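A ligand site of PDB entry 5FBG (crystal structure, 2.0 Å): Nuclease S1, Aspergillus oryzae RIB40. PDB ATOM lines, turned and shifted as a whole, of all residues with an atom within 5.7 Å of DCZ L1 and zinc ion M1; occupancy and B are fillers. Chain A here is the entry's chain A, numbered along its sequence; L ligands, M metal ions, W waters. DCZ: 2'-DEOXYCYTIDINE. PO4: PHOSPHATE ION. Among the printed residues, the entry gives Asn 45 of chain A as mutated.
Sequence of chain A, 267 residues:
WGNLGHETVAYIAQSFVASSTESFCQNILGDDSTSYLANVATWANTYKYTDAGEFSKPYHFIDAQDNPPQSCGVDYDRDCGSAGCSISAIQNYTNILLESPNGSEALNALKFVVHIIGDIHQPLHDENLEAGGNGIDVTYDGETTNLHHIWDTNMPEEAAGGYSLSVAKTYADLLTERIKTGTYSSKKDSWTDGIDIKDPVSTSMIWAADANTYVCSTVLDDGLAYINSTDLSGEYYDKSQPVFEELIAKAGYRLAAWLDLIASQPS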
ATOM      1  N   TRP A   1      -5.086   9.300   8.142  1.00  0.00           N
ATOM      2  CA  TRP A   1      -5.616   9.890   9.330  1.00  0.00           C
ATOM      3  C   TRP A   1      -7.064   9.453   9.519  1.00  0.00           C
ATOM      4  O   TRP A   1      -7.756   9.128   8.547  1.00  0.00           O
ATOM      5  CB  TRP A   1      -5.555  11.415   9.333  1.00  0.00           C
ATOM      6  CG  TRP A   1      -4.193  11.964   9.000  1.00  0.00           C
ATOM      7  CD1 TRP A   1      -3.808  12.468   7.826  1.00  0.00           C
ATOM      8  CD2 TRP A   1      -3.041  12.042   9.885  1.00  0.00           C
ATOM      9  NE1 TRP A   1      -2.508  12.932   7.919  1.00  0.00           N
ATOM     10  CE2 TRP A   1      -2.027  12.671   9.184  1.00  0.00           C
ATOM     11  CE3 TRP A   1      -2.816  11.658  11.217  1.00  0.00           C
ATOM     12  CZ2 TRP A   1      -0.735  12.877   9.738  1.00  0.00           C
ATOM     13  CZ3 TRP A   1      -1.558  11.889  11.779  1.00  0.00           C
ATOM     14  CH2 TRP A   1      -0.525  12.489  11.041  1.00  0.00           C
ATOM     15  N   GLY A   2      -7.515   9.586  10.765  1.00  0.00           N
ATOM     16  CA  GLY A   2      -8.935   9.540  11.079  1.00  0.00           C
ATOM     17  C   GLY A   2      -9.593  10.885  10.716  1.00  0.00           C
ATOM     18  O   GLY A   2      -8.981  11.770  10.102  1.00  0.00           O
ATOM     19  N   ASN A  45     -12.598   7.980   2.214  1.00  0.00           N
ATOM     20  CA  ASN A  45     -12.780   6.858   3.081  1.00  0.00           C
ATOM     21  C   ASN A  45     -14.170   6.264   2.959  1.00  0.00           C
ATOM     22  O   ASN A  45     -14.323   5.067   2.785  1.00  0.00           O
ATOM     23  CB  ASN A  45     -12.447   7.166   4.543  1.00  0.00           C
ATOM     24  CG  ASN A  45     -10.956   7.183   4.810  1.00  0.00           C
ATOM     25  OD1 ASN A  45     -10.173   6.780   3.972  1.00  0.00           O
ATOM     26  ND2 ASN A  45     -10.586   7.693   5.942  1.00  0.00           N
ATOM     27  N   LYS A  48     -14.505   4.368  -0.471  1.00  0.00           N
ATOM     28  CA  LYS A  48     -13.747   3.107  -0.653  1.00  0.00           C
ATOM     29  C   LYS A  48     -14.520   1.856  -0.101  1.00  0.00           C
ATOM     30  O   LYS A  48     -14.226   0.725  -0.523  1.00  0.00           O
ATOM     31  CB  LYS A  48     -12.347   3.182  -0.069  1.00  0.00           C
ATOM     32  CG  LYS A  48     -12.297   3.034   1.445  1.00  0.00           C
ATOM     33  CD  LYS A  48     -10.902   3.420   1.923  1.00  0.00           C
ATOM     34  CE  LYS A  48     -10.611   3.280   3.393  1.00  0.00           C
ATOM     35  NZ  LYS A  48      -9.252   3.853   3.751  1.00  0.00           N
ATOM     36  N   TYR A  49     -15.477   2.086   0.818  1.00  0.00           N
ATOM     37  CA  TYR A  49     -16.308   1.039   1.379  1.00  0.00           C
ATOM     38  C   TYR A  49     -17.650   0.775   0.659  1.00  0.00           C
ATOM     39  O   TYR A  49     -18.438  -0.068   1.101  1.00  0.00           O
ATOM     40  CB  TYR A  49     -16.530   1.263   2.872  1.00  0.00           C
ATOM     41  CG  TYR A  49     -15.238   1.411   3.674  1.00  0.00           C
ATOM     42  CD1 TYR A  49     -14.330   0.383   3.741  1.00  0.00           C
ATOM     43  CD2 TYR A  49     -14.994   2.568   4.439  1.00  0.00           C
ATOM     44  CE1 TYR A  49     -13.180   0.468   4.504  1.00  0.00           C
ATOM     45  CE2 TYR A  49     -13.850   2.651   5.253  1.00  0.00           C
ATOM     46  CZ  TYR A  49     -12.948   1.595   5.255  1.00  0.00           C
ATOM     47  OH  TYR A  49     -11.799   1.680   6.018  1.00  0.00           O
ATOM     48  N   LYS A  57      -9.530   1.700  -2.690  1.00  0.00           N
ATOM     49  CA  LYS A  57      -8.860   1.435  -1.433  1.00  0.00           C
ATOM     50  C   LYS A  57      -7.317   1.609  -1.429  1.00  0.00           C
ATOM     51  O   LYS A  57      -6.779   2.117  -0.479  1.00  0.00           O
ATOM     52  CB  LYS A  57      -9.184   0.011  -0.898  1.00  0.00           C
ATOM     53  CG  LYS A  57     -10.542  -0.084  -0.205  1.00  0.00           C
ATOM     54  CD  LYS A  57     -10.891  -1.532   0.172  1.00  0.00           C
ATOM     55  CE  LYS A  57     -12.277  -1.523   0.790  1.00  0.00           C
ATOM     56  NZ  LYS A  57     -12.666  -2.874   1.280  1.00  0.00           N
ATOM     57  N   HIS A  60      -5.013   5.168  -0.916  1.00  0.00           N
ATOM     58  CA  HIS A  60      -4.798   5.869   0.335  1.00  0.00           C
ATOM     59  C   HIS A  60      -3.399   5.787   0.901  1.00  0.00           C
ATOM     60  O   HIS A  60      -3.078   6.468   1.939  1.00  0.00           O
ATOM     61  CB  HIS A  60      -5.815   5.330   1.379  1.00  0.00           C
ATOM     62  CG  HIS A  60      -7.217   5.681   1.018  1.00  0.00           C
ATOM     63  ND1 HIS A  60      -7.982   6.550   1.773  1.00  0.00           N
ATOM     64  CD2 HIS A  60      -7.932   5.408  -0.108  1.00  0.00           C
ATOM     65  CE1 HIS A  60      -9.141   6.731   1.171  1.00  0.00           C
ATOM     66  NE2 HIS A  60      -9.124   6.089   0.006  1.00  0.00           N
ATOM     67  N   PHE A  61      -2.547   4.974   0.266  1.00  0.00           N
ATOM     68  CA  PHE A  61      -1.201   4.708   0.810  1.00  0.00           C
ATOM     69  C   PHE A  61      -0.246   4.312  -0.287  1.00  0.00           C
ATOM     70  O   PHE A  61      -0.600   4.090  -1.458  1.00  0.00           O
ATOM     71  CB  PHE A  61      -1.284   3.656   1.953  1.00  0.00           C
ATOM     72  CG  PHE A  61      -1.958   2.390   1.528  1.00  0.00           C
ATOM     73  CD1 PHE A  61      -1.245   1.399   0.846  1.00  0.00           C
ATOM     74  CD2 PHE A  61      -3.316   2.192   1.802  1.00  0.00           C
ATOM     75  CE1 PHE A  61      -1.868   0.250   0.433  1.00  0.00           C
ATOM     76  CE2 PHE A  61      -3.962   1.033   1.402  1.00  0.00           C
ATOM     77  CZ  PHE A  61      -3.254   0.062   0.711  1.00  0.00           C
ATOM     78  N   ASP A  63       2.871   1.472  -0.216  1.00  0.00           N
ATOM     79  CA  ASP A  63       3.492   0.467   0.656  1.00  0.00           C
ATOM     80  C   ASP A  63       5.023   0.366   0.439  1.00  0.00           C
ATOM     81  O   ASP A  63       5.542  -0.571  -0.236  1.00  0.00           O
ATOM     82  CB  ASP A  63       2.827  -0.882   0.442  1.00  0.00           C
ATOM     83  CG  ASP A  63       1.553  -1.064   1.279  1.00  0.00           C
ATOM     84  OD1 ASP A  63       1.377  -0.445   2.328  1.00  0.00           O
ATOM     85  OD2 ASP A  63       0.722  -1.916   0.867  1.00  0.00           O
ATOM     86  N   ASP A 119      -3.506  11.967   3.732  1.00  0.00           N
ATOM     87  CA  ASP A 119      -3.059  10.576   4.056  1.00  0.00           C
ATOM     88  C   ASP A 119      -1.551  10.355   3.796  1.00  0.00           C
ATOM     89  O   ASP A 119      -0.878   9.724   4.605  1.00  0.00           O
ATOM     90  CB  ASP A 119      -3.844   9.563   3.245  1.00  0.00           C
ATOM     91  CG  ASP A 119      -5.016   8.966   3.953  1.00  0.00           C
ATOM     92  OD1 ASP A 119      -5.239   9.223   5.177  1.00  0.00           O
ATOM     93  OD2 ASP A 119      -5.752   8.263   3.225  1.00  0.00           O
ATOM     94  N   GLN A 122       0.683  11.008   6.785  1.00  0.00           N
ATOM     95  CA  GLN A 122       0.628  10.110   7.914  1.00  0.00           C
ATOM     96  C   GLN A 122       1.714   9.048   7.623  1.00  0.00           C
ATOM     97  O   GLN A 122       1.565   8.311   6.659  1.00  0.00           O
ATOM     98  CB  GLN A 122      -0.762   9.461   8.027  1.00  0.00           C
ATOM     99  CG  GLN A 122      -1.159   9.003   9.416  1.00  0.00           C
ATOM    100  CD  GLN A 122      -0.462   7.675   9.877  1.00  0.00           C
ATOM    101  OE1 GLN A 122       0.772   7.640  10.002  1.00  0.00           O
ATOM    102  NE2 GLN A 122      -1.234   6.661  10.137  1.00  0.00           N
ATOM    103  N   LEU A 124       2.774   6.139   8.495  1.00  0.00           N
ATOM    104  CA  LEU A 124       2.385   4.736   8.250  1.00  0.00           C
ATOM    105  C   LEU A 124       1.579   4.470   6.970  1.00  0.00           C
ATOM    106  O   LEU A 124       1.418   3.314   6.537  1.00  0.00           O
ATOM    107  CB  LEU A 124       1.726   4.129   9.460  1.00  0.00           C
ATOM    108  CG  LEU A 124       2.717   3.762  10.591  1.00  0.00           C
ATOM    109  CD1 LEU A 124       1.989   3.402  11.872  1.00  0.00           C
ATOM    110  CD2 LEU A 124       3.636   2.600  10.158  1.00  0.00           C
ATOM    111  N   HIS A 125       1.125   5.549   6.314  1.00  0.00           N
ATOM    112  CA  HIS A 125       0.587   5.460   4.921  1.00  0.00           C
ATOM    113  C   HIS A 125       1.665   5.446   3.876  1.00  0.00           C
ATOM    114  O   HIS A 125       1.376   5.459   2.681  1.00  0.00           O
ATOM    115  CB  HIS A 125      -0.341   6.679   4.690  1.00  0.00           C
ATOM    116  CG  HIS A 125      -1.709   6.495   5.282  1.00  0.00           C
ATOM    117  ND1 HIS A 125      -2.818   6.318   4.487  1.00  0.00           N
ATOM    118  CD2 HIS A 125      -2.126   6.403   6.551  1.00  0.00           C
ATOM    119  CE1 HIS A 125      -3.866   6.109   5.256  1.00  0.00           C
ATOM    120  NE2 HIS A 125      -3.479   6.178   6.505  1.00  0.00           N
ATOM    121  N   GLU A 127       4.460   3.083   4.180  1.00  0.00           N
ATOM    122  CA  GLU A 127       5.194   1.979   4.775  1.00  0.00           C
ATOM    123  C   GLU A 127       4.471   0.636   4.588  1.00  0.00           C
ATOM    124  O   GLU A 127       3.283   0.506   4.938  1.00  0.00           O
ATOM    125  CB  GLU A 127       5.416   2.231   6.257  1.00  0.00           C
ATOM    126  CG  GLU A 127       6.111   1.084   6.996  1.00  0.00           C
ATOM    127  CD  GLU A 127       7.437   0.696   6.316  1.00  0.00           C
ATOM    128  OE1 GLU A 127       8.190   1.629   6.036  1.00  0.00           O
ATOM    129  OE2 GLU A 127       7.659  -0.507   6.017  1.00  0.00           O
ATOM    130  N   ASN A 128       5.183  -0.333   4.014  1.00  0.00           N
ATOM    131  CA  ASN A 128       4.584  -1.657   3.754  1.00  0.00           C
ATOM    132  C   ASN A 128       4.363  -2.489   4.992  1.00  0.00           C
ATOM    133  O   ASN A 128       3.340  -3.188   5.115  1.00  0.00           O
ATOM    134  CB  ASN A 128       5.413  -2.436   2.748  1.00  0.00           C
ATOM    135  CG  ASN A 128       4.720  -3.693   2.311  1.00  0.00           C
ATOM    136  OD1 ASN A 128       3.616  -3.670   1.807  1.00  0.00           O
ATOM    137  ND2 ASN A 128       5.377  -4.824   2.516  1.00  0.00           N
ATOM    138  N   ALA A 131       0.933  -4.153   6.800  1.00  0.00           N
ATOM    139  CA  ALA A 131      -0.101  -3.338   6.190  1.00  0.00           C
ATOM    140  C   ALA A 131      -0.166  -1.924   6.761  1.00  0.00           C
ATOM    141  O   ALA A 131      -1.190  -1.540   7.326  1.00  0.00           O
ATOM    142  CB  ALA A 131      -1.449  -4.060   6.319  1.00  0.00           C
ATOM    143  N   GLY A 132       0.962  -1.211   6.682  1.00  0.00           N
ATOM    144  CA  GLY A 132       1.070   0.115   7.261  1.00  0.00           C
ATOM    145  C   GLY A 132       0.891   0.172   8.776  1.00  0.00           C
ATOM    146  O   GLY A 132       0.363   1.127   9.325  1.00  0.00           O
ATOM    147  N   ASN A 134      -1.049  -1.756  10.475  1.00  0.00           N
ATOM    148  CA  ASN A 134      -2.355  -2.273  10.916  1.00  0.00           C
ATOM    149  C   ASN A 134      -2.247  -3.598  11.677  1.00  0.00           C
ATOM    150  O   ASN A 134      -3.003  -3.844  12.579  1.00  0.00           O
ATOM    151  CB  ASN A 134      -3.331  -2.387   9.745  1.00  0.00           C
ATOM    152  CG  ASN A 134      -4.011  -1.030   9.430  1.00  0.00           C
ATOM    153  OD1 ASN A 134      -4.863  -0.556  10.200  1.00  0.00           O
ATOM    154  ND2 ASN A 134      -3.576  -0.380   8.349  1.00  0.00           N
ATOM    155  N   ASN A 146      -4.270  -0.857  17.304  1.00  0.00           N
ATOM    156  CA  ASN A 146      -3.061  -1.152  16.535  1.00  0.00           C
ATOM    157  C   ASN A 146      -2.303   0.118  16.251  1.00  0.00           C
ATOM    158  O   ASN A 146      -2.805   1.245  16.455  1.00  0.00           O
ATOM    159  CB  ASN A 146      -3.396  -1.920  15.265  1.00  0.00           C
ATOM    160  CG  ASN A 146      -4.234  -1.084  14.294  1.00  0.00           C
ATOM    161  OD1 ASN A 146      -3.702  -0.169  13.640  1.00  0.00           O
ATOM    162  ND2 ASN A 146      -5.542  -1.384  14.206  1.00  0.00           N
ATOM    163  N   HIS A 148      -1.166   1.568  13.525  1.00  0.00           N
ATOM    164  CA  HIS A 148      -1.671   2.437  12.492  1.00  0.00           C
ATOM    165  C   HIS A 148      -2.799   3.329  13.085  1.00  0.00           C
ATOM    166  O   HIS A 148      -2.827   4.562  12.888  1.00  0.00           O
ATOM    167  CB  HIS A 148      -2.231   1.654  11.336  1.00  0.00           C
ATOM    168  CG  HIS A 148      -2.648   2.511  10.187  1.00  0.00           C
ATOM    169  ND1 HIS A 148      -1.865   2.662   9.056  1.00  0.00           N
ATOM    170  CD2 HIS A 148      -3.729   3.313  10.005  1.00  0.00           C
ATOM    171  CE1 HIS A 148      -2.469   3.514   8.219  1.00  0.00           C
ATOM    172  NE2 HIS A 148      -3.609   3.875   8.761  1.00  0.00           N
ATOM    173  N   HIS A 149      -3.681   2.692  13.844  1.00  0.00           N
ATOM    174  CA  HIS A 149      -4.836   3.383  14.417  1.00  0.00           C
ATOM    175  C   HIS A 149      -4.490   4.487  15.384  1.00  0.00           C
ATOM    176  O   HIS A 149      -5.141   5.558  15.390  1.00  0.00           O
ATOM    177  CB  HIS A 149      -5.793   2.396  15.078  1.00  0.00           C
ATOM    178  CG  HIS A 149      -7.145   2.974  15.384  1.00  0.00           C
ATOM    179  ND1 HIS A 149      -7.459   3.568  16.586  1.00  0.00           N
ATOM    180  CD2 HIS A 149      -8.275   3.040  14.635  1.00  0.00           C
ATOM    181  CE1 HIS A 149      -8.721   3.955  16.578  1.00  0.00           C
ATOM    182  NE2 HIS A 149      -9.228   3.658  15.402  1.00  0.00           N
ATOM    183  N   ASP A 152      -3.371   7.415  13.273  1.00  0.00           N
ATOM    184  CA  ASP A 152      -4.487   7.997  12.535  1.00  0.00           C
ATOM    185  C   ASP A 152      -5.400   8.830  13.477  1.00  0.00           C
ATOM    186  O   ASP A 152      -5.822   9.926  13.123  1.00  0.00           O
ATOM    187  CB  ASP A 152      -5.350   6.917  11.871  1.00  0.00           C
ATOM    188  CG  ASP A 152      -5.023   6.648  10.407  1.00  0.00           C
ATOM    189  OD1 ASP A 152      -4.060   7.145   9.821  1.00  0.00           O
ATOM    190  OD2 ASP A 152      -5.752   5.813   9.835  1.00  0.00           O
HETATM  191  N1  DCZ L   1      -3.758   1.329   5.323  1.00  0.00           N
HETATM  192  C2  DCZ L   1      -2.463   1.765   5.016  1.00  0.00           C
HETATM  193  N3  DCZ L   1      -1.574   0.874   4.462  1.00  0.00           N
HETATM  194  C4  DCZ L   1      -1.960  -0.374   4.175  1.00  0.00           C
HETATM  195  C5  DCZ L   1      -3.288  -0.846   4.490  1.00  0.00           C
HETATM  196  C6  DCZ L   1      -4.139   0.017   5.072  1.00  0.00           C
HETATM  197  O2  DCZ L   1      -2.187   2.951   5.182  1.00  0.00           O
HETATM  198  N4  DCZ L   1      -1.100  -1.176   3.579  1.00  0.00           N
HETATM  199  C1' DCZ L   1      -4.739   2.311   5.831  1.00  0.00           C
HETATM  200  C2' DCZ L   1      -6.007   2.443   4.980  1.00  0.00           C
HETATM  201  C3' DCZ L   1      -7.073   1.657   5.775  1.00  0.00           C
HETATM  202  C4' DCZ L   1      -6.585   1.841   7.201  1.00  0.00           C
HETATM  203  O4' DCZ L   1      -5.140   1.880   7.110  1.00  0.00           O
HETATM  204  O3' DCZ L   1      -8.415   2.159   5.763  1.00  0.00           O
HETATM  205  C5' DCZ L   1      -7.010   0.769   8.199  1.00  0.00           C
HETATM  206  O5' DCZ L   1      -6.742   1.289   9.513  1.00  0.00           O
HETATM  207  P   PO4 L   2      -7.448   6.148   6.136  1.00  0.00           P
HETATM  208  O1  PO4 L   2      -7.597   7.649   6.134  1.00  0.00           O
HETATM  209  O2  PO4 L   2      -7.222   5.696   4.688  1.00  0.00           O
HETATM  210  O3  PO4 L   2      -6.351   5.674   7.032  1.00  0.00           O
HETATM  211  O4  PO4 L   2      -8.642   5.330   6.571  1.00  0.00           O
HETATM  212 ZN    ZN M   1      -4.788   5.475   8.044  1.00  0.00          ZN
HETATM  213 ZN    ZN M   2      -6.647   9.095   6.680  1.00  0.00          ZN
HETATM  214 ZN    ZN M   3      -7.689   7.431   3.613  1.00  0.00          ZN
HETATM  215  O   HOH W   1     -10.087  -0.360   5.949  1.00  0.00           O
HETATM  216  O   HOH W   2      -1.764  -3.546   2.493  1.00  0.00           O
HETATM  217  O   HOH W   3      -7.348   0.405  12.525  1.00  0.00           O
HETATM  218  O   HOH W   4       1.004   1.920   4.145  1.00  0.00           O
HETATM  219  O   HOH W   5      -7.467   2.267   2.086  1.00  0.00           O
HETATM  220  O   HOH W   6      -7.216   3.522  11.557  1.00  0.00           O
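A ring nitrogen (ND1) of His 125 lies within hydrogen-bond range of an oxygen (O2) of DCZ L1, at 3.5 Å.
The side-chain hydroxyl (OH) of Tyr 49 is in hydrogen-bond range of an oxygen (O3') of DCZ L1 (3.4 Å).
NZ of Lys 48 is in hydrogen-bond range of O3' of DCZ L1.
An oxygen (O5') of DCZ L1 sits at hydrogen-bond distance from the side-chain amide oxygen of Asn 134 (2.7 Å).
OD1 of Asp 63 is in hydrogen-bond range of N4 of DCZ L1, at 2.9 Å.
A ring nitrogen (NE2) of His 148 sits close to an oxygen (O4') of DCZ L1, 3.0 Å away.
A ring nitrogen (ND1) of His 148 sits at hydrogen-bond distance from the backbone carbonyl oxygen (O) of Gly 132, 2.7 Å away.
The side-chain carboxylate (OD1) of Asp 152 sits close to the side-chain amide nitrogen (NE2) of Gln 122, at 2.9 Å.
ND2 of Asn 134 is in hydrogen-bond range of O of Ala 131, 2.8 Å away.
NZ of Lys 48 sits close to OD1 of Asn 45, at 3.1 Å.
The backbone NH (N) of His 148 is in hydrogen-bond range of the side-chain amide oxygen (OD1) of Asn 146, 3.1 Å away.
O of His 60 sits at hydrogen-bond distance from ND1 of His 125.
The backbone NH (N) of Leu 124 is in hydrogen-bond range of the side-chain amide oxygen (OE1) of Gln 122 (2.9 Å).
O of Glu 127 sits close to N of Gly 132 (3.4 Å).
Phe 61 touches DCZ L1 (CG to N3, 3.3 Å).
O of Leu 124 touches O2 of DCZ L1, at 3.9 Å.
Ala 131 touches DCZ L1.
Gly 132 touches DCZ L1 (N to N4, 3.7 Å).
Hydrophobic or aromatic side chains that line DCZ L1: Phe 61, His 125, Ala 131 and His 148.
Of the 22 residues printed, 10 come within 4 Å of DCZ L1.
Trp 1 touches zinc ion M1 (N to ZN, 3.8 Å).
Of the 22 residues printed, 4 come within 4 Å of zinc ion M1.
Along chain A the residues within 4 Å of zinc ion M1 span positions 1 to 152.
Zinc ion M1 is bound by an oxygen (O3) of PO4 L2 (1.9 Å), the side-chain carboxylate (OD2) of Asp 152 (2.1 Å), a ring nitrogen (NE2) of His 148 (2.1 Å), a ring nitrogen (NE2) of His 125 (2.1 Å) and the side-chain carboxylate (OD1) of Asp 152 (2.5 Å).
Water W2 bridges N4 of DCZ L1 and OD2 of Asp 63.
Water W1 lies within hydrogen-bond range of OH of Tyr 49 and O3' of DCZ L1.
Water W3 lies within hydrogen-bond range of ND2 of Asn 146 (3.0 Å) and O5' of DCZ L1 (3.2 Å).
Water W5 lies within hydrogen-bond range of O of Lys 57 (2.7 Å) and NZ of Lys 48 (2.9 Å).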
